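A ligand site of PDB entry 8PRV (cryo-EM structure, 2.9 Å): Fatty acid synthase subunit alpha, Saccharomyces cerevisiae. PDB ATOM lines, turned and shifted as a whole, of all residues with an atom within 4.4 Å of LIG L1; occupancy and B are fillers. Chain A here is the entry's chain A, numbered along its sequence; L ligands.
The side-chain hydroxyl (OG1) of Thr 875 sits at hydrogen-bond distance from the backbone NH (N) of Met 878, at 3.4 Å. OG1 of Thr 875 lies close to N of Leu 877 (3.5 Å). The backbone carbonyl oxygen of Pro 825 sits at hydrogen-bond distance from the side-chain amino group of Lys 843 (2.8 Å). The backbone carbonyl oxygen (O) of Ile 794 sits at hydrogen-bond distance from the side-chain amide nitrogen (NE2) of Gln 739, at 3.0 Å. The backbone NH of Gly 740 is in hydrogen-bond range of the side-chain amide oxygen of Asn 738 (2.8 Å). OG1 of Thr 872 sits at hydrogen-bond distance from O of Gly 870 (2.7 Å). The backbone NH (N) of Arg 709 is in hydrogen-bond range of the side-chain hydroxyl (OG1) of Thr 707 (3.3 Å). OG of Ser 687 sits close to N of Gly 689 (3.5 Å).
Merely in contact with LIG L1: Gly 682 (3.4 Å), Gly 684 (3.6 Å), Ser 687 (3.5 Å), Thr 706 (3.97 Å), Phe 737 (3.7 Å), Phe 771 (3.3 Å), Ala 772 (3.4 Å), Ile 774 (3.4 Å), Ile 794 (3.8 Å), Pro 825 (3.4 Å), Met 826 (3.7 Å), Ile 869 (3.4 Å), Gly 870 (3.6 Å), Leu 877 (3.5 Å) and Met 878 (3.3 Å). Within 4 Å of LIG L1: Gly 682, Gly 684, Ser 687, Ile 688, Thr 706, Thr 707, Ser 708, Arg 709, Phe 737, Asn 738, Gln 739, Phe 771, Ala 772, Ala 773, Ile 774, Ile 794, Pro 825, Met 826, Tyr 839, Lys 843, Ile 869, Gly 870, Thr 872, Thr 875, Gly 876, Leu 877 and Met 878. The nearest printed residue that does not touch LIG L1 is Trp 871 (4.03 Å).
N of Ser 708 is in hydrogen-bond range of O17 of LIG L1 (2.7 Å). The side-chain hydroxyl (OG) of Ser 708 is in hydrogen-bond range of an oxygen (O17) of LIG L1 (2.6 Å). An oxygen (O8) of LIG L1 lies within hydrogen-bond range of the side-chain hydroxyl (OG1) of Thr 875 (2.6 Å). The side-chain amino group (NZ) of Lys 843 is in hydrogen-bond range of an oxygen (O13) of LIG L1. The side-chain hydroxyl (OH) of Tyr 839 is in hydrogen-bond range of an oxygen (O13) of LIG L1 (2.8 Å). A nitrogen (N4) of LIG L1 lies within hydrogen-bond range of the backbone NH of Gln 739, 2.9 Å away. The backbone NH (N) of Gly 876 sits at hydrogen-bond distance from an oxygen (O1) of LIG L1 (2.9 Å). The side-chain amide oxygen (OD1) of Asn 738 is in hydrogen-bond range of a nitrogen (N3) of LIG L1, 3.1 Å away. O of Thr 872 sits close to N7 of LIG L1 (3.4 Å). An oxygen (O15) of LIG L1 is in salt-bridge range of the guanidinium group (NH2) of Arg 709, at 3.1 Å. The backbone NH (N) of Ile 688 is in hydrogen-bond range of an oxygen (O9) of LIG L1 (3.1 Å). An oxygen (O16) of LIG L1 sits at hydrogen-bond distance from the side-chain hydroxyl of Thr 707, at 3.4 Å. O4 of LIG L1 is in hydrogen-bond range of N of Ala 773, 3.5 Å away. The side-chain hydroxyl (OG) of Ser 827 is in hydrogen-bond range of an oxygen (O1) of LG2 L2, at 2.5 Å.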
ATOM      1  N   GLY A 682       1.604  -3.184 -14.820  1.00  0.00           N
ATOM      2  CA  GLY A 682       0.277  -2.781 -14.327  1.00  0.00           C
ATOM      3  C   GLY A 682       0.276  -1.407 -13.687  1.00  0.00           C
ATOM      4  O   GLY A 682      -0.206  -1.286 -12.528  1.00  0.00           O
ATOM      5  N   GLY A 684      -1.146   1.287 -15.446  1.00  0.00           N
ATOM      6  CA  GLY A 684      -2.094   1.979 -16.333  1.00  0.00           C
ATOM      7  C   GLY A 684      -2.895   3.029 -15.593  1.00  0.00           C
ATOM      8  O   GLY A 684      -2.936   2.976 -14.374  1.00  0.00           O
ATOM      9  N   SER A 687      -4.989   2.739 -11.927  1.00  0.00           N
ATOM     10  CA  SER A 687      -4.397   1.662 -11.116  1.00  0.00           C
ATOM     11  C   SER A 687      -3.697   2.209  -9.873  1.00  0.00           C
ATOM     12  O   SER A 687      -3.502   3.456  -9.744  1.00  0.00           O
ATOM     13  CB  SER A 687      -3.425   0.915 -11.955  1.00  0.00           C
ATOM     14  OG  SER A 687      -2.387   1.783 -12.349  1.00  0.00           O
ATOM     15  N   ILE A 688      -3.348   1.282  -8.989  1.00  0.00           N
ATOM     16  CA  ILE A 688      -2.402   1.507  -7.879  1.00  0.00           C
ATOM     17  C   ILE A 688      -1.067   1.858  -8.510  1.00  0.00           C
ATOM     18  O   ILE A 688      -0.492   2.868  -8.128  1.00  0.00           O
ATOM     19  CB  ILE A 688      -2.314   0.259  -6.974  1.00  0.00           C
ATOM     20  CG1 ILE A 688      -3.641   0.049  -6.239  1.00  0.00           C
ATOM     21  CG2 ILE A 688      -1.192   0.346  -5.966  1.00  0.00           C
ATOM     22  CD1 ILE A 688      -3.715  -1.272  -5.513  1.00  0.00           C
ATOM     23  N   GLY A 689      -0.610   1.046  -9.442  1.00  0.00           N
ATOM     24  CA  GLY A 689       0.724   1.143 -10.047  1.00  0.00           C
ATOM     25  C   GLY A 689       1.006   2.493 -10.638  1.00  0.00           C
ATOM     26  O   GLY A 689       2.185   2.855 -10.657  1.00  0.00           O
ATOM     27  N   THR A 706       5.725  -0.766 -18.007  1.00  0.00           N
ATOM     28  CA  THR A 706       5.239  -1.571 -19.144  1.00  0.00           C
ATOM     29  C   THR A 706       3.789  -1.207 -19.399  1.00  0.00           C
ATOM     30  O   THR A 706       3.135  -0.771 -18.469  1.00  0.00           O
ATOM     31  CB  THR A 706       5.299  -3.049 -18.863  1.00  0.00           C
ATOM     32  OG1 THR A 706       4.145  -3.271 -18.038  1.00  0.00           O
ATOM     33  CG2 THR A 706       6.617  -3.494 -18.248  1.00  0.00           C
ATOM     34  N   THR A 707       3.297  -1.456 -20.594  1.00  0.00           N
ATOM     35  CA  THR A 707       1.889  -1.229 -20.931  1.00  0.00           C
ATOM     36  C   THR A 707       1.473  -2.321 -21.889  1.00  0.00           C
ATOM     37  O   THR A 707       2.262  -2.666 -22.747  1.00  0.00           O
ATOM     38  CB  THR A 707       1.665   0.207 -21.410  1.00  0.00           C
ATOM     39  OG1 THR A 707       0.314   0.378 -21.815  1.00  0.00           O
ATOM     40  CG2 THR A 707       2.606   0.607 -22.539  1.00  0.00           C
ATOM     41  N   SER A 708       0.305  -2.899 -21.682  1.00  0.00           N
ATOM     42  CA  SER A 708      -0.285  -3.847 -22.655  1.00  0.00           C
ATOM     43  C   SER A 708      -0.816  -3.065 -23.871  1.00  0.00           C
ATOM     44  O   SER A 708      -0.651  -3.581 -24.996  1.00  0.00           O
ATOM     45  CB  SER A 708      -1.326  -4.709 -21.996  1.00  0.00           C
ATOM     46  OG  SER A 708      -2.561  -4.036 -21.803  1.00  0.00           O
ATOM     47  N   ARG A 709      -1.356  -1.864 -23.648  1.00  0.00           N
ATOM     48  CA  ARG A 709      -2.175  -1.068 -24.591  1.00  0.00           C
ATOM     49  C   ARG A 709      -1.315   0.060 -25.162  1.00  0.00           C
ATOM     50  O   ARG A 709      -1.711   1.216 -25.041  1.00  0.00           O
ATOM     51  CB  ARG A 709      -3.421  -0.514 -23.869  1.00  0.00           C
ATOM     52  CG  ARG A 709      -4.596  -1.485 -23.770  1.00  0.00           C
ATOM     53  CD  ARG A 709      -5.795  -0.934 -23.007  1.00  0.00           C
ATOM     54  NE  ARG A 709      -5.687  -1.164 -21.562  1.00  0.00           N
ATOM     55  CZ  ARG A 709      -5.847  -2.344 -20.924  1.00  0.00           C
ATOM     56  NH1 ARG A 709      -6.119  -3.454 -21.590  1.00  0.00           N
ATOM     57  NH2 ARG A 709      -5.713  -2.400 -19.610  1.00  0.00           N
ATOM     58  N   TYR A 718       2.115   8.979 -20.144  1.00  0.00           N
ATOM     59  CA  TYR A 718       3.375   8.769 -19.388  1.00  0.00           C
ATOM     60  C   TYR A 718       4.297   9.948 -19.620  1.00  0.00           C
ATOM     61  O   TYR A 718       5.021  10.318 -18.686  1.00  0.00           O
ATOM     62  CB  TYR A 718       4.062   7.485 -19.828  1.00  0.00           C
ATOM     63  CG  TYR A 718       3.390   6.273 -19.259  1.00  0.00           C
ATOM     64  CD1 TYR A 718       3.289   6.095 -17.883  1.00  0.00           C
ATOM     65  CD2 TYR A 718       2.828   5.332 -20.082  1.00  0.00           C
ATOM     66  CE1 TYR A 718       2.651   4.994 -17.329  1.00  0.00           C
ATOM     67  CE2 TYR A 718       2.190   4.225 -19.541  1.00  0.00           C
ATOM     68  CZ  TYR A 718       2.071   4.060 -18.162  1.00  0.00           C
ATOM     69  OH  TYR A 718       1.438   2.944 -17.700  1.00  0.00           O
ATOM     70  N   PHE A 737       4.354  -4.509 -23.654  1.00  0.00           N
ATOM     71  CA  PHE A 737       4.611  -5.745 -22.890  1.00  0.00           C
ATOM     72  C   PHE A 737       3.292  -6.419 -22.585  1.00  0.00           C
ATOM     73  O   PHE A 737       2.371  -5.755 -22.155  1.00  0.00           O
ATOM     74  CB  PHE A 737       5.298  -5.397 -21.589  1.00  0.00           C
ATOM     75  CG  PHE A 737       5.591  -6.525 -20.654  1.00  0.00           C
ATOM     76  CD1 PHE A 737       6.551  -7.461 -20.980  1.00  0.00           C
ATOM     77  CD2 PHE A 737       4.962  -6.594 -19.412  1.00  0.00           C
ATOM     78  CE1 PHE A 737       6.872  -8.469 -20.079  1.00  0.00           C
ATOM     79  CE2 PHE A 737       5.310  -7.565 -18.502  1.00  0.00           C
ATOM     80  CZ  PHE A 737       6.257  -8.517 -18.837  1.00  0.00           C
ATOM     81  N   ASN A 738       3.271  -7.716 -22.814  1.00  0.00           N
ATOM     82  CA  ASN A 738       2.167  -8.613 -22.432  1.00  0.00           C
ATOM     83  C   ASN A 738       2.704  -9.531 -21.358  1.00  0.00           C
ATOM     84  O   ASN A 738       3.574 -10.313 -21.703  1.00  0.00           O
ATOM     85  CB  ASN A 738       1.722  -9.402 -23.643  1.00  0.00           C
ATOM     86  CG  ASN A 738       0.595 -10.338 -23.313  1.00  0.00           C
ATOM     87  OD1 ASN A 738       0.143 -10.435 -22.173  1.00  0.00           O
ATOM     88  ND2 ASN A 738       0.154 -11.057 -24.308  1.00  0.00           N
ATOM     89  N   GLN A 739       2.259  -9.396 -20.121  1.00  0.00           N
ATOM     90  CA  GLN A 739       2.808 -10.253 -19.041  1.00  0.00           C
ATOM     91  C   GLN A 739       2.374 -11.692 -19.324  1.00  0.00           C
ATOM     92  O   GLN A 739       3.068 -12.587 -18.892  1.00  0.00           O
ATOM     93  CB  GLN A 739       2.375  -9.737 -17.668  1.00  0.00           C
ATOM     94  CG  GLN A 739       3.208 -10.318 -16.514  1.00  0.00           C
ATOM     95  CD  GLN A 739       3.149  -9.430 -15.296  1.00  0.00           C
ATOM     96  OE1 GLN A 739       3.650  -8.298 -15.292  1.00  0.00           O
ATOM     97  NE2 GLN A 739       2.509  -9.895 -14.229  1.00  0.00           N
ATOM     98  N   GLY A 740       1.277 -11.884 -20.052  1.00  0.00           N
ATOM     99  CA  GLY A 740       0.750 -13.214 -20.426  1.00  0.00           C
ATOM    100  C   GLY A 740       1.731 -14.016 -21.242  1.00  0.00           C
ATOM    101  O   GLY A 740       1.796 -15.204 -21.071  1.00  0.00           O
ATOM    102  N   PHE A 771       2.435  -5.680 -11.003  1.00  0.00           N
ATOM    103  CA  PHE A 771       1.052  -5.359 -10.630  1.00  0.00           C
ATOM    104  C   PHE A 771       0.096  -5.552 -11.784  1.00  0.00           C
ATOM    105  O   PHE A 771      -1.027  -5.125 -11.672  1.00  0.00           O
ATOM    106  CB  PHE A 771       0.989  -3.932 -10.089  1.00  0.00           C
ATOM    107  CG  PHE A 771       1.320  -3.759  -8.636  1.00  0.00           C
ATOM    108  CD1 PHE A 771       1.931  -4.766  -7.892  1.00  0.00           C
ATOM    109  CD2 PHE A 771       1.074  -2.546  -8.018  1.00  0.00           C
ATOM    110  CE1 PHE A 771       2.247  -4.565  -6.551  1.00  0.00           C
ATOM    111  CE2 PHE A 771       1.390  -2.350  -6.689  1.00  0.00           C
ATOM    112  CZ  PHE A 771       1.950  -3.360  -5.944  1.00  0.00           C
ATOM    113  N   ALA A 772       0.498  -6.157 -12.892  1.00  0.00           N
ATOM    114  CA  ALA A 772      -0.424  -6.464 -13.999  1.00  0.00           C
ATOM    115  C   ALA A 772      -1.480  -7.418 -13.479  1.00  0.00           C
ATOM    116  O   ALA A 772      -1.214  -8.134 -12.467  1.00  0.00           O
ATOM    117  CB  ALA A 772       0.301  -7.105 -15.143  1.00  0.00           C
ATOM    118  N   ALA A 773      -2.609  -7.430 -14.150  1.00  0.00           N
ATOM    119  CA  ALA A 773      -3.855  -8.084 -13.693  1.00  0.00           C
ATOM    120  C   ALA A 773      -4.950  -7.770 -14.695  1.00  0.00           C
ATOM    121  O   ALA A 773      -5.038  -6.599 -15.095  1.00  0.00           O
ATOM    122  CB  ALA A 773      -4.234  -7.557 -12.339  1.00  0.00           C
ATOM    123  N   ILE A 774      -5.752  -8.742 -15.080  1.00  0.00           N
ATOM    124  CA  ILE A 774      -7.037  -8.479 -15.797  1.00  0.00           C
ATOM    125  C   ILE A 774      -8.186  -8.783 -14.862  1.00  0.00           C
ATOM    126  O   ILE A 774      -8.107  -9.715 -14.070  1.00  0.00           O
ATOM    127  CB  ILE A 774      -7.139  -9.244 -17.113  1.00  0.00           C
ATOM    128  CG1 ILE A 774      -7.024 -10.742 -16.930  1.00  0.00           C
ATOM    129  CG2 ILE A 774      -6.104  -8.719 -18.109  1.00  0.00           C
ATOM    130  CD1 ILE A 774      -6.978 -11.472 -18.229  1.00  0.00           C
ATOM    131  N   ILE A 794      -0.816 -14.635 -16.256  1.00  0.00           N
ATOM    132  CA  ILE A 794      -0.398 -13.235 -16.004  1.00  0.00           C
ATOM    133  C   ILE A 794      -0.043 -13.034 -14.524  1.00  0.00           C
ATOM    134  O   ILE A 794       0.998 -12.458 -14.250  1.00  0.00           O
ATOM    135  CB  ILE A 794      -1.512 -12.260 -16.366  1.00  0.00           C
ATOM    136  CG1 ILE A 794      -1.778 -12.233 -17.869  1.00  0.00           C
ATOM    137  CG2 ILE A 794      -1.184 -10.886 -15.845  1.00  0.00           C
ATOM    138  CD1 ILE A 794      -3.059 -11.525 -18.216  1.00  0.00           C
ATOM    139  N   PRO A 825       1.981  -8.344  -5.027  1.00  0.00           N
ATOM    140  CA  PRO A 825       0.670  -7.756  -4.761  1.00  0.00           C
ATOM    141  C   PRO A 825      -0.260  -8.860  -4.270  1.00  0.00           C
ATOM    142  O   PRO A 825      -0.960  -9.451  -5.060  1.00  0.00           O
ATOM    143  CB  PRO A 825       0.249  -7.276  -6.159  1.00  0.00           C
ATOM    144  CG  PRO A 825       0.870  -8.310  -7.121  1.00  0.00           C
ATOM    145  CD  PRO A 825       2.104  -8.834  -6.421  1.00  0.00           C
ATOM    146  N   MET A 826      -0.209  -9.137  -2.973  1.00  0.00           N
ATOM    147  CA  MET A 826      -1.032 -10.195  -2.324  1.00  0.00           C
ATOM    148  C   MET A 826      -2.378  -9.620  -1.916  1.00  0.00           C
ATOM    149  O   MET A 826      -2.506  -8.415  -1.926  1.00  0.00           O
ATOM    150  CB  MET A 826      -0.316 -10.713  -1.098  1.00  0.00           C
ATOM    151  CG  MET A 826       0.723 -11.691  -1.483  1.00  0.00           C
ATOM    152  SD  MET A 826       1.875 -11.925  -0.154  1.00  0.00           S
ATOM    153  CE  MET A 826       2.784 -13.268  -0.918  1.00  0.00           C
ATOM    154  N   SER A 827      -3.331 -10.464  -1.607  1.00  0.00           N
ATOM    155  CA  SER A 827      -4.716 -10.049  -1.349  1.00  0.00           C
ATOM    156  C   SER A 827      -5.247 -10.765  -0.125  1.00  0.00           C
ATOM    157  O   SER A 827      -4.743 -11.831   0.215  1.00  0.00           O
ATOM    158  CB  SER A 827      -5.573 -10.323  -2.529  1.00  0.00           C
ATOM    159  OG  SER A 827      -6.940 -10.245  -2.187  1.00  0.00           O
ATOM    160  N   TYR A 839      -8.654 -15.694  -9.457  1.00  0.00           N
ATOM    161  CA  TYR A 839      -7.947 -14.540  -8.873  1.00  0.00           C
ATOM    162  C   TYR A 839      -7.452 -15.033  -7.522  1.00  0.00           C
ATOM    163  O   TYR A 839      -6.273 -15.134  -7.315  1.00  0.00           O
ATOM    164  CB  TYR A 839      -8.840 -13.300  -8.837  1.00  0.00           C
ATOM    165  CG  TYR A 839      -8.255 -12.127  -8.101  1.00  0.00           C
ATOM    166  CD1 TYR A 839      -8.408 -12.006  -6.732  1.00  0.00           C
ATOM    167  CD2 TYR A 839      -7.547 -11.137  -8.754  1.00  0.00           C
ATOM    168  CE1 TYR A 839      -7.854 -10.951  -6.017  1.00  0.00           C
ATOM    169  CE2 TYR A 839      -6.999 -10.068  -8.068  1.00  0.00           C
ATOM    170  CZ  TYR A 839      -7.147  -9.966  -6.684  1.00  0.00           C
ATOM    171  OH  TYR A 839      -6.598  -8.932  -5.968  1.00  0.00           O
ATOM    172  N   LYS A 843      -3.453 -15.106  -6.081  1.00  0.00           N
ATOM    173  CA  LYS A 843      -3.066 -14.350  -4.872  1.00  0.00           C
ATOM    174  C   LYS A 843      -2.590 -15.310  -3.782  1.00  0.00           C
ATOM    175  O   LYS A 843      -1.628 -14.988  -3.078  1.00  0.00           O
ATOM    176  CB  LYS A 843      -4.274 -13.556  -4.384  1.00  0.00           C
ATOM    177  CG  LYS A 843      -4.819 -12.530  -5.372  1.00  0.00           C
ATOM    178  CD  LYS A 843      -3.862 -11.396  -5.638  1.00  0.00           C
ATOM    179  CE  LYS A 843      -3.105 -11.575  -6.916  1.00  0.00           C
ATOM    180  NZ  LYS A 843      -2.449 -10.308  -7.301  1.00  0.00           N
ATOM    181  N   ILE A 869      -2.451  -6.126   0.083  1.00  0.00           N
ATOM    182  CA  ILE A 869      -3.070  -4.823  -0.278  1.00  0.00           C
ATOM    183  C   ILE A 869      -4.534  -4.910   0.100  1.00  0.00           C
ATOM    184  O   ILE A 869      -5.147  -5.952  -0.171  1.00  0.00           O
ATOM    185  CB  ILE A 869      -2.864  -4.531  -1.775  1.00  0.00           C
ATOM    186  CG1 ILE A 869      -1.393  -4.326  -2.071  1.00  0.00           C
ATOM    187  CG2 ILE A 869      -3.673  -3.343  -2.206  1.00  0.00           C
ATOM    188  CD1 ILE A 869      -1.008  -4.633  -3.476  1.00  0.00           C
ATOM    189  N   GLY A 870      -5.058  -3.860   0.713  1.00  0.00           N
ATOM    190  CA  GLY A 870      -6.470  -3.795   1.075  1.00  0.00           C
ATOM    191  C   GLY A 870      -7.341  -3.291  -0.063  1.00  0.00           C
ATOM    192  O   GLY A 870      -6.820  -2.917  -1.132  1.00  0.00           O
ATOM    193  N   TRP A 871      -8.630  -3.275   0.191  1.00  0.00           N
ATOM    194  CA  TRP A 871      -9.649  -2.682  -0.695  1.00  0.00           C
ATOM    195  C   TRP A 871      -9.170  -1.305  -1.142  1.00  0.00           C
ATOM    196  O   TRP A 871      -9.026  -0.447  -0.306  1.00  0.00           O
ATOM    197  CB  TRP A 871     -10.940  -2.586   0.084  1.00  0.00           C
ATOM    198  CG  TRP A 871     -12.129  -2.197  -0.729  1.00  0.00           C
ATOM    199  CD1 TRP A 871     -12.292  -1.146  -1.585  1.00  0.00           C
ATOM    200  CD2 TRP A 871     -13.374  -2.862  -0.648  1.00  0.00           C
ATOM    201  NE1 TRP A 871     -13.576  -1.124  -2.051  1.00  0.00           N
ATOM    202  CE2 TRP A 871     -14.264  -2.165  -1.491  1.00  0.00           C
ATOM    203  CE3 TRP A 871     -13.808  -4.007   0.033  1.00  0.00           C
ATOM    204  CZ2 TRP A 871     -15.569  -2.596  -1.697  1.00  0.00           C
ATOM    205  CZ3 TRP A 871     -15.102  -4.436  -0.181  1.00  0.00           C
ATOM    206  CH2 TRP A 871     -15.969  -3.730  -1.027  1.00  0.00           C
ATOM    207  N   THR A 872      -8.981  -1.109  -2.441  1.00  0.00           N
ATOM    208  CA  THR A 872      -8.418   0.116  -3.023  1.00  0.00           C
ATOM    209  C   THR A 872      -9.354   0.566  -4.117  1.00  0.00           C
ATOM    210  O   THR A 872      -9.434  -0.095  -5.125  1.00  0.00           O
ATOM    211  CB  THR A 872      -7.027  -0.058  -3.609  1.00  0.00           C
ATOM    212  OG1 THR A 872      -6.244  -0.707  -2.611  1.00  0.00           O
ATOM    213  CG2 THR A 872      -6.418   1.277  -4.007  1.00  0.00           C
ATOM    214  N   THR A 875      -9.847   1.235  -8.997  1.00  0.00           N
ATOM    215  CA  THR A 875      -8.920   0.499  -9.871  1.00  0.00           C
ATOM    216  C   THR A 875      -9.696  -0.327 -10.902  1.00  0.00           C
ATOM    217  O   THR A 875     -10.919  -0.336 -10.867  1.00  0.00           O
ATOM    218  CB  THR A 875      -7.932  -0.334  -9.056  1.00  0.00           C
ATOM    219  OG1 THR A 875      -8.616  -1.431  -8.442  1.00  0.00           O
ATOM    220  CG2 THR A 875      -7.216   0.501  -8.020  1.00  0.00           C
ATOM    221  N   GLY A 876      -8.989  -0.961 -11.828  1.00  0.00           N
ATOM    222  CA  GLY A 876      -9.610  -1.901 -12.781  1.00  0.00           C
ATOM    223  C   GLY A 876     -10.347  -2.994 -12.032  1.00  0.00           C
ATOM    224  O   GLY A 876     -11.501  -3.305 -12.392  1.00  0.00           O
ATOM    225  N   LEU A 877      -9.719  -3.532 -11.005  1.00  0.00           N
ATOM    226  CA  LEU A 877     -10.235  -4.718 -10.300  1.00  0.00           C
ATOM    227  C   LEU A 877     -11.358  -4.353  -9.317  1.00  0.00           C
ATOM    228  O   LEU A 877     -12.095  -5.266  -8.954  1.00  0.00           O
ATOM    229  CB  LEU A 877      -9.069  -5.424  -9.588  1.00  0.00           C
ATOM    230  CG  LEU A 877      -8.242  -6.319 -10.490  1.00  0.00           C
ATOM    231  CD1 LEU A 877      -6.926  -6.651  -9.829  1.00  0.00           C
ATOM    232  CD2 LEU A 877      -8.977  -7.605 -10.839  1.00  0.00           C
ATOM    233  N   MET A 878     -11.505  -3.098  -8.904  1.00  0.00           N
ATOM    234  CA  MET A 878     -12.398  -2.744  -7.776  1.00  0.00           C
ATOM    235  C   MET A 878     -13.338  -1.577  -8.062  1.00  0.00           C
ATOM    236  O   MET A 878     -14.038  -1.203  -7.100  1.00  0.00           O
ATOM    237  CB  MET A 878     -11.567  -2.416  -6.534  1.00  0.00           C
ATOM    238  CG  MET A 878     -11.035  -3.653  -5.865  1.00  0.00           C
ATOM    239  SD  MET A 878     -12.342  -4.747  -5.260  1.00  0.00           S
ATOM    240  CE  MET A 878     -12.423  -4.122  -3.583  1.00  0.00           C
HETATM  241  P1  LIG L   1      -5.689  -2.666 -12.327  1.00  0.00           P
HETATM  242  O1  LIG L   1      -6.123  -1.298 -11.994  1.00  0.00           O
HETATM  243  O2  LIG L   1      -6.516  -3.556 -13.272  1.00  0.00           O
HETATM  244  O3  LIG L   1      -4.249  -2.605 -12.938  1.00  0.00           O
HETATM  245  C1  LIG L   1      -3.777  -3.720 -13.686  1.00  0.00           C
HETATM  246  C2  LIG L   1      -3.101  -3.174 -14.954  1.00  0.00           C
HETATM  247  O4  LIG L   1      -2.472  -4.265 -15.587  1.00  0.00           O
HETATM  248  C3  LIG L   1      -4.026  -2.651 -16.016  1.00  0.00           C
HETATM  249  O5  LIG L   1      -4.290  -1.278 -15.630  1.00  0.00           O
HETATM  250  C4  LIG L   1      -3.244  -2.852 -17.276  1.00  0.00           C
HETATM  251  O6  LIG L   1      -2.461  -1.690 -17.595  1.00  0.00           O
HETATM  252  C5  LIG L   1      -2.272  -3.926 -16.913  1.00  0.00           C
HETATM  253  N1  LIG L   1      -2.440  -5.133 -17.700  1.00  0.00           N
HETATM  254  C6  LIG L   1      -3.564  -5.774 -17.994  1.00  0.00           C
HETATM  255  N2  LIG L   1      -3.315  -6.847 -18.784  1.00  0.00           N
HETATM  256  C7  LIG L   1      -1.995  -6.868 -18.936  1.00  0.00           C
HETATM  257  C8  LIG L   1      -1.097  -7.720 -19.633  1.00  0.00           C
HETATM  258  N3  LIG L   1      -1.591  -8.762 -20.299  1.00  0.00           N
HETATM  259  N4  LIG L   1       0.199  -7.456 -19.573  1.00  0.00           N
HETATM  260  C9  LIG L   1       0.654  -6.400 -18.898  1.00  0.00           C
HETATM  261  N5  LIG L   1      -0.133  -5.529 -18.261  1.00  0.00           N
HETATM  262  C10 LIG L   1      -1.435  -5.738 -18.244  1.00  0.00           C
HETATM  263  O7  LIG L   1      -5.225  -3.510 -11.070  1.00  0.00           O
HETATM  264  P2  LIG L   1      -5.000  -2.812  -9.672  1.00  0.00           P
HETATM  265  O8  LIG L   1      -6.432  -2.636  -9.302  1.00  0.00           O
HETATM  266  O9  LIG L   1      -4.004  -1.677  -9.702  1.00  0.00           O
HETATM  267  O10 LIG L   1      -4.309  -3.918  -8.780  1.00  0.00           O
HETATM  268  C11 LIG L   1      -2.973  -4.204  -9.115  1.00  0.00           C
HETATM  269  C12 LIG L   1      -2.406  -5.405  -8.414  1.00  0.00           C
HETATM  270  O11 LIG L   1      -2.661  -5.222  -7.026  1.00  0.00           O
HETATM  271  C13 LIG L   1      -3.041  -6.695  -8.867  1.00  0.00           C
HETATM  272  O12 LIG L   1      -2.024  -7.701  -8.851  1.00  0.00           O
HETATM  273  C14 LIG L   1      -4.081  -6.965  -7.822  1.00  0.00           C
HETATM  274  O13 LIG L   1      -4.318  -8.316  -7.498  1.00  0.00           O
HETATM  275  C15 LIG L   1      -3.446  -6.351  -6.607  1.00  0.00           C
HETATM  276  N6  LIG L   1      -4.461  -5.974  -5.665  1.00  0.00           N
HETATM  277  C16 LIG L   1      -5.340  -5.020  -5.963  1.00  0.00           C
HETATM  278  C17 LIG L   1      -6.299  -4.678  -5.037  1.00  0.00           C
HETATM  279  C18 LIG L   1      -7.237  -3.608  -5.428  1.00  0.00           C
HETATM  280  O14 LIG L   1      -7.224  -3.138  -6.558  1.00  0.00           O
HETATM  281  N7  LIG L   1      -8.050  -3.120  -4.559  1.00  0.00           N
HETATM  282  C19 LIG L   1      -6.342  -5.295  -3.786  1.00  0.00           C
HETATM  283  C20 LIG L   1      -5.409  -6.292  -3.508  1.00  0.00           C
HETATM  284  C21 LIG L   1      -4.461  -6.612  -4.482  1.00  0.00           C
HETATM  285  P3  LIG L   1      -2.022  -1.209 -19.106  1.00  0.00           P
HETATM  286  O15 LIG L   1      -3.273  -0.520 -19.598  1.00  0.00           O
HETATM  287  O16 LIG L   1      -0.798  -0.341 -18.734  1.00  0.00           O
HETATM  288  O17 LIG L   1      -1.780  -2.443 -19.952  1.00  0.00           O
HETATM  289  C1  LG2 L   2      -9.852  -7.827  -5.149  1.00  0.00           C
HETATM  290  C2  LG2 L   2      -8.926  -6.827  -4.491  1.00  0.00           C
HETATM  291  C3  LG2 L   2      -8.711  -7.240  -3.046  1.00  0.00           C
HETATM  292  C4  LG2 L   2      -9.614  -6.699  -1.963  1.00  0.00           C
HETATM  293  O1  LG2 L   2      -7.789  -7.999  -2.804  1.00  0.00           O
HETATM  294  O2  LG2 L   2     -10.304  -8.768  -4.496  1.00  0.00           O
HETATM  295  O3  LG2 L   2     -15.402  -8.017  -6.988  1.00  0.00           O
HETATM  296  C5  LG2 L   2     -14.989  -9.160  -7.046  1.00  0.00           C
HETATM  297  N1  LG2 L   2     -13.729  -9.525  -6.846  1.00  0.00           N
HETATM  298  C6  LG2 L   2     -12.687  -8.544  -6.591  1.00  0.00           C
HETATM  299  C7  LG2 L   2     -11.397  -8.844  -7.355  1.00  0.00           C
HETATM  300  S1  LG2 L   2     -10.222  -7.668  -6.790  1.00  0.00           S
HETATM  301  C8  LG2 L   2     -15.934 -10.248  -7.470  1.00  0.00           C
HETATM  302  C9  LG2 L   2     -15.925 -10.193  -9.011  1.00  0.00           C
HETATM  303  N2  LG2 L   2     -16.880  -9.203  -9.515  1.00  0.00           N
HETATM  304  C10 LG2 L   2     -18.113  -9.518  -9.913  1.00  0.00           C
HETATM  305  O4  LG2 L   2     -18.543 -10.661  -9.942  1.00  0.00           O
HETATM  306  C11 LG2 L   2     -19.045  -8.408 -10.298  1.00  0.00           C
HETATM  307  O5  LG2 L   2     -18.312  -7.371 -11.016  1.00  0.00           O
HETATM  308  C12 LG2 L   2     -19.886  -7.904  -9.077  1.00  0.00           C
HETATM  309  C13 LG2 L   2     -20.449  -9.039  -8.195  1.00  0.00           C
HETATM  310  C14 LG2 L   2     -19.072  -6.957  -8.208  1.00  0.00           C
HETATM  311  C15 LG2 L   2     -21.143  -7.221  -9.628  1.00  0.00           C
HETATM  312  O6  LG2 L   2     -20.930  -6.368 -10.774  1.00  0.00           O
HETATM  313  P1  LG2 L   2     -22.240  -5.688 -11.423  1.00  0.00           P
HETATM  314  O7  LG2 L   2     -22.656  -6.356 -12.798  1.00  0.00           O
HETATM  315  O8  LG2 L   2     -23.475  -5.998 -10.571  1.00  0.00           O
HETATM  316  O9  LG2 L   2     -21.970  -4.214 -11.615  1.00  0.00           O
